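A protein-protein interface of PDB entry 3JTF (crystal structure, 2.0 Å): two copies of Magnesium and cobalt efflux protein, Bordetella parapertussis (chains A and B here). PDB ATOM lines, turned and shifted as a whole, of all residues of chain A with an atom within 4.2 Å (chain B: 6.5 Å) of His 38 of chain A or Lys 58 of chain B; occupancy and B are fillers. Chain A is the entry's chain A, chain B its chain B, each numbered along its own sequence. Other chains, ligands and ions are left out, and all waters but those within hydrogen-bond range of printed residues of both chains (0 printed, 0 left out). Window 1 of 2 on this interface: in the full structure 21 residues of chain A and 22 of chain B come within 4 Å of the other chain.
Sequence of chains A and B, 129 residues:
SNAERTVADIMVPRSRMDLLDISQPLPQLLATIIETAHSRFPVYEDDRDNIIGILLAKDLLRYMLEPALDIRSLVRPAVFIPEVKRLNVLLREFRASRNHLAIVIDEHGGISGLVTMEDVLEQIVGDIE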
ATOM      1  N   ASP A  18      12.441  16.886  16.482  1.00  0.00           N
ATOM      2  CA  ASP A  18      12.646  16.377  15.121  1.00  0.00           C
ATOM      3  C   ASP A  18      11.536  16.948  14.245  1.00  0.00           C
ATOM      4  O   ASP A  18      10.391  16.521  14.351  1.00  0.00           O
ATOM      5  CB  ASP A  18      12.662  14.856  15.116  1.00  0.00           C
ATOM      6  CG  ASP A  18      13.882  14.301  15.819  1.00  0.00           C
ATOM      7  OD1 ASP A  18      14.986  14.849  15.652  1.00  0.00           O
ATOM      8  OD2 ASP A  18      13.734  13.363  16.606  1.00  0.00           O
ATOM      9  N   ILE A  33      12.281  10.378   8.662  1.00  0.00           N
ATOM     10  CA  ILE A  33      11.243   9.662   9.389  1.00  0.00           C
ATOM     11  C   ILE A  33      11.681   8.243   9.840  1.00  0.00           C
ATOM     12  O   ILE A  33      11.336   7.798  10.939  1.00  0.00           O
ATOM     13  CB  ILE A  33       9.953   9.603   8.577  1.00  0.00           C
ATOM     14  CG1 ILE A  33       9.301  10.995   8.554  1.00  0.00           C
ATOM     15  CG2 ILE A  33       8.977   8.586   9.155  1.00  0.00           C
ATOM     16  CD1 ILE A  33       8.559  11.275   7.292  1.00  0.00           C
ATOM     17  N   THR A  36      14.627   8.035  12.824  1.00  0.00           N
ATOM     18  CA  THR A  36      14.376   8.578  14.150  1.00  0.00           C
ATOM     19  C   THR A  36      13.250   7.774  14.772  1.00  0.00           C
ATOM     20  O   THR A  36      12.302   7.359  14.093  1.00  0.00           O
ATOM     21  CB  THR A  36      14.081  10.100  14.123  1.00  0.00           C
ATOM     22  OG1 THR A  36      12.693  10.332  13.900  1.00  0.00           O
ATOM     23  CG2 THR A  36      14.897  10.800  13.035  1.00  0.00           C
ATOM     24  N   ALA A  37      13.373   7.516  16.064  1.00  0.00           N
ATOM     25  CA  ALA A  37      12.384   6.736  16.774  1.00  0.00           C
ATOM     26  C   ALA A  37      11.286   7.660  17.291  1.00  0.00           C
ATOM     27  O   ALA A  37      11.153   7.822  18.503  1.00  0.00           O
ATOM     28  CB  ALA A  37      13.048   5.968  17.942  1.00  0.00           C
ATOM     29  N   HIS A  38      10.528   8.282  16.383  1.00  0.00           N
ATOM     30  CA  HIS A  38       9.314   9.040  16.729  1.00  0.00           C
ATOM     31  C   HIS A  38       8.148   8.713  15.828  1.00  0.00           C
ATOM     32  O   HIS A  38       8.327   8.428  14.665  1.00  0.00           O
ATOM     33  CB  HIS A  38       9.570  10.544  16.661  1.00  0.00           C
ATOM     34  CG  HIS A  38      10.544  11.015  17.680  1.00  0.00           C
ATOM     35  ND1 HIS A  38      10.378  10.779  19.031  1.00  0.00           N
ATOM     36  CD2 HIS A  38      11.726  11.656  17.548  1.00  0.00           C
ATOM     37  CE1 HIS A  38      11.414  11.272  19.688  1.00  0.00           C
ATOM     38  NE2 HIS A  38      12.239  11.819  18.813  1.00  0.00           N
ATOM     39  N   SER A  39       6.941   8.792  16.380  1.00  0.00           N
ATOM     40  CA  SER A  39       5.744   8.523  15.646  1.00  0.00           C
ATOM     41  C   SER A  39       5.176   9.807  14.996  1.00  0.00           C
ATOM     42  O   SER A  39       4.583   9.730  13.930  1.00  0.00           O
ATOM     43  CB  SER A  39       4.702   7.861  16.565  1.00  0.00           C
ATOM     44  OG  SER A  39       4.289   8.742  17.617  1.00  0.00           O
ATOM     45  N   ARG A  40       5.372  10.959  15.641  1.00  0.00           N
ATOM     46  CA  ARG A  40       4.775  12.226  15.248  1.00  0.00           C
ATOM     47  C   ARG A  40       5.880  13.273  15.041  1.00  0.00           C
ATOM     48  O   ARG A  40       6.849  13.319  15.789  1.00  0.00           O
ATOM     49  CB  ARG A  40       3.788  12.747  16.330  1.00  0.00           C
ATOM     50  CG  ARG A  40       2.627  11.794  16.702  1.00  0.00           C
ATOM     51  CD  ARG A  40       2.142  12.035  18.166  1.00  0.00           C
ATOM     52  NE  ARG A  40       3.133  11.612  19.191  1.00  0.00           N
ATOM     53  CZ  ARG A  40       2.866  11.502  20.498  1.00  0.00           C
ATOM     54  NH1 ARG A  40       1.661  11.814  20.970  1.00  0.00           N
ATOM     55  NH2 ARG A  40       3.796  11.102  21.344  1.00  0.00           N
ATOM     56  N   PHE A  41       5.714  14.094  14.017  1.00  0.00           N
ATOM     57  CA  PHE A  41       6.669  15.116  13.653  1.00  0.00           C
ATOM     58  C   PHE A  41       5.934  16.407  13.362  1.00  0.00           C
ATOM     59  O   PHE A  41       5.070  16.449  12.489  1.00  0.00           O
ATOM     60  CB  PHE A  41       7.410  14.725  12.375  1.00  0.00           C
ATOM     61  CG  PHE A  41       8.167  13.473  12.479  1.00  0.00           C
ATOM     62  CD1 PHE A  41       7.534  12.249  12.383  1.00  0.00           C
ATOM     63  CD2 PHE A  41       9.542  13.508  12.657  1.00  0.00           C
ATOM     64  CE1 PHE A  41       8.255  11.065  12.472  1.00  0.00           C
ATOM     65  CE2 PHE A  41      10.271  12.344  12.751  1.00  0.00           C
ATOM     66  CZ  PHE A  41       9.632  11.113  12.658  1.00  0.00           C
ATOM     67  N   ALA A  57       3.809   9.572  11.296  1.00  0.00           N
ATOM     68  CA  ALA A  57       4.611   8.772  10.396  1.00  0.00           C
ATOM     69  C   ALA A  57       3.777   7.739   9.653  1.00  0.00           C
ATOM     70  O   ALA A  57       3.932   7.537   8.437  1.00  0.00           O
ATOM     71  CB  ALA A  57       5.737   8.083  11.152  1.00  0.00           C
ATOM     72  N   SER B  39       0.507   2.426  16.302  1.00  0.00           N
ATOM     73  CA  SER B  39       1.797   2.457  15.617  1.00  0.00           C
ATOM     74  C   SER B  39       2.467   1.076  15.559  1.00  0.00           C
ATOM     75  O   SER B  39       3.352   0.869  14.746  1.00  0.00           O
ATOM     76  CB  SER B  39       2.752   3.426  16.320  1.00  0.00           C
ATOM     77  OG  SER B  39       2.814   3.139  17.734  1.00  0.00           O
ATOM     78  N   LEU B  55       5.461  -5.557  14.558  1.00  0.00           N
ATOM     79  CA  LEU B  55       5.777  -4.697  13.424  1.00  0.00           C
ATOM     80  C   LEU B  55       5.486  -3.260  13.829  1.00  0.00           C
ATOM     81  O   LEU B  55       4.398  -2.959  14.316  1.00  0.00           O
ATOM     82  CB  LEU B  55       4.935  -5.048  12.194  1.00  0.00           C
ATOM     83  CG  LEU B  55       5.178  -4.173  10.935  1.00  0.00           C
ATOM     84  CD1 LEU B  55       6.596  -4.465  10.360  1.00  0.00           C
ATOM     85  CD2 LEU B  55       4.127  -4.507   9.909  1.00  0.00           C
ATOM     86  N   LEU B  56       6.483  -2.399  13.662  1.00  0.00           N
ATOM     87  CA  LEU B  56       6.291  -0.953  13.748  1.00  0.00           C
ATOM     88  C   LEU B  56       5.843  -0.469  12.362  1.00  0.00           C
ATOM     89  O   LEU B  56       6.552  -0.627  11.377  1.00  0.00           O
ATOM     90  CB  LEU B  56       7.607  -0.292  14.191  1.00  0.00           C
ATOM     91  CG  LEU B  56       7.639   1.228  14.399  1.00  0.00           C
ATOM     92  CD1 LEU B  56       6.819   1.728  15.644  1.00  0.00           C
ATOM     93  CD2 LEU B  56       9.123   1.718  14.472  1.00  0.00           C
ATOM     94  N   ALA B  57       4.653   0.109  12.290  1.00  0.00           N
ATOM     95  CA  ALA B  57       4.025   0.506  11.018  1.00  0.00           C
ATOM     96  C   ALA B  57       4.936   1.347  10.132  1.00  0.00           C
ATOM     97  O   ALA B  57       4.956   1.145   8.926  1.00  0.00           O
ATOM     98  CB  ALA B  57       2.767   1.306  11.271  1.00  0.00           C
ATOM     99  N   LYS B  58       5.679   2.262  10.741  1.00  0.00           N
ATOM    100  CA  LYS B  58       6.499   3.186   9.990  1.00  0.00           C
ATOM    101  C   LYS B  58       7.652   2.483   9.247  1.00  0.00           C
ATOM    102  O   LYS B  58       8.127   2.983   8.214  1.00  0.00           O
ATOM    103  CB  LYS B  58       7.011   4.315  10.891  1.00  0.00           C
ATOM    104  CG  LYS B  58       8.078   3.943  11.863  1.00  0.00           C
ATOM    105  CD  LYS B  58       8.424   5.151  12.790  1.00  0.00           C
ATOM    106  CE  LYS B  58       9.784   5.777  12.472  1.00  0.00           C
ATOM    107  NZ  LYS B  58       9.833   7.235  12.958  1.00  0.00           N
ATOM    108  N   ASP B  59       8.054   1.313   9.727  1.00  0.00           N
ATOM    109  CA  ASP B  59       9.040   0.510   9.017  1.00  0.00           C
ATOM    110  C   ASP B  59       8.592   0.078   7.628  1.00  0.00           C
ATOM    111  O   ASP B  59       9.445  -0.179   6.751  1.00  0.00           O
ATOM    112  CB  ASP B  59       9.480  -0.690   9.856  1.00  0.00           C
ATOM    113  CG  ASP B  59      10.502  -0.309  10.934  1.00  0.00           C
ATOM    114  OD1 ASP B  59      11.217   0.671  10.689  1.00  0.00           O
ATOM    115  OD2 ASP B  59      10.626  -1.001  11.984  1.00  0.00           O
ATOM    116  N   LEU B  60       7.291   0.021   7.382  1.00  0.00           N
ATOM    117  CA  LEU B  60       6.847  -0.343   6.039  1.00  0.00           C
ATOM    118  C   LEU B  60       7.215   0.737   5.000  1.00  0.00           C
ATOM    119  O   LEU B  60       7.174   0.470   3.800  1.00  0.00           O
ATOM    120  CB  LEU B  60       5.343  -0.659   5.994  1.00  0.00           C
ATOM    121  CG  LEU B  60       4.900  -2.000   6.606  1.00  0.00           C
ATOM    122  CD1 LEU B  60       3.398  -2.180   6.397  1.00  0.00           C
ATOM    123  CD2 LEU B  60       5.654  -3.161   5.958  1.00  0.00           C
ATOM    124  N   LEU B  61       7.582   1.937   5.451  1.00  0.00           N
ATOM    125  CA  LEU B  61       8.073   2.972   4.534  1.00  0.00           C
ATOM    126  C   LEU B  61       9.370   2.566   3.836  1.00  0.00           C
ATOM    127  O   LEU B  61       9.722   3.142   2.826  1.00  0.00           O
ATOM    128  CB  LEU B  61       8.296   4.298   5.254  1.00  0.00           C
ATOM    129  CG  LEU B  61       6.993   4.935   5.716  1.00  0.00           C
ATOM    130  CD1 LEU B  61       7.343   6.071   6.760  1.00  0.00           C
ATOM    131  CD2 LEU B  61       6.176   5.439   4.528  1.00  0.00           C
ATOM    132  N   ARG B  62      10.071   1.589   4.386  1.00  0.00           N
ATOM    133  CA  ARG B  62      11.263   1.051   3.730  1.00  0.00           C
ATOM    134  C   ARG B  62      10.996   0.382   2.383  1.00  0.00           C
ATOM    135  O   ARG B  62      11.921   0.148   1.625  1.00  0.00           O
ATOM    136  CB  ARG B  62      11.946   0.084   4.659  1.00  0.00           C
ATOM    137  CG  ARG B  62      12.512   0.738   5.889  1.00  0.00           C
ATOM    138  CD  ARG B  62      12.967  -0.331   6.851  1.00  0.00           C
ATOM    139  NE  ARG B  62      13.353   0.172   8.165  1.00  0.00           N
ATOM    140  CZ  ARG B  62      14.564   0.608   8.508  1.00  0.00           C
ATOM    141  NH1 ARG B  62      15.545   0.642   7.629  1.00  0.00           N
ATOM    142  NH2 ARG B  62      14.787   1.015   9.757  1.00  0.00           N
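Of the printed residues of chain B, Thr 36 of chain A touches Lys 58 (2.7 Å). Ala 37 of chain A touches none of the printed residues of chain B. His 38 of chain A touches just one residue of chain B: Lys 58. Printed residues of chain B within 4 Å of Phe 41 of chain A: Lys 58 (3.9 Å). Printed residues of chain B within 4 Å of Ala 57 of chain A: Lys 58 (3.99 Å). Of the printed residues of chain A, Lys 58 of chain B touches Ile 33 (2.6 Å), Thr 36 (2.7 Å), His 38 (2.6 Å), Phe 41 (3.9 Å) and Ala 57 (3.99 Å). Of the printed residues of chain A, Leu 61 of chain B touches Ile 33 (3.8 Å). The nearest printed residue of chain A that does not touch Lys 58 of chain B is Ala 37 of chain A (4.6 Å). The nearest printed residue of chain B that does not touch Ile 33 of chain A is Asp 59 of chain B (7.1 Å).
O of Ile 33 of chain A is in hydrogen-bond range of NZ of Lys 58 of chain B, 2.6 Å away. O of Thr 36 of chain A is in hydrogen-bond range of NZ of Lys 58 of chain B (2.7 Å). The backbone carbonyl oxygen of His 38 of chain A sits at hydrogen-bond distance from the side-chain amino group of Lys 58 of chain B, 2.6 Å away.
2 positions are printed for both chains. Of the 6 pairs that touch across the chains among the printed residues, none has its exchanged pair printed and touching as well.
Of the 9 printed residues of chain B, 2 touch a printed residue of chain A. Printed residues of chain B that touch a printed residue of chain A: Lys 58 and Leu 61. Hydrophobic or aromatic side chains of chain B that line the printed part of chain A: Leu 61. Hydrophobic or aromatic side chains of chain A within 4 Å of the printed part of chain B: Ile 33, Phe 41 and Ala 57. Among the printed residues, no Asp or Glu carboxylate lies within 4 Å of a Lys or Arg side-chain nitrogen of the other chain.
The side-chain carboxylate (OD2) of Asp 18 of chain A sits close to a ring nitrogen (NE2) of His 38 of chain A (3.1 Å). N of Ala 57 of chain A lies within hydrogen-bond range of O of Ser 39 of chain A, 2.7 Å away.
CD1 of Leu 61 of chain B touches CG2 of Ile 33 of chain A, at 3.8 Å. CZ of Phe 41 of chain A touches NZ of Lys 58 of chain B, at 3.9 Å. Ala 57 of chain A touches Lys 58 of chain B.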
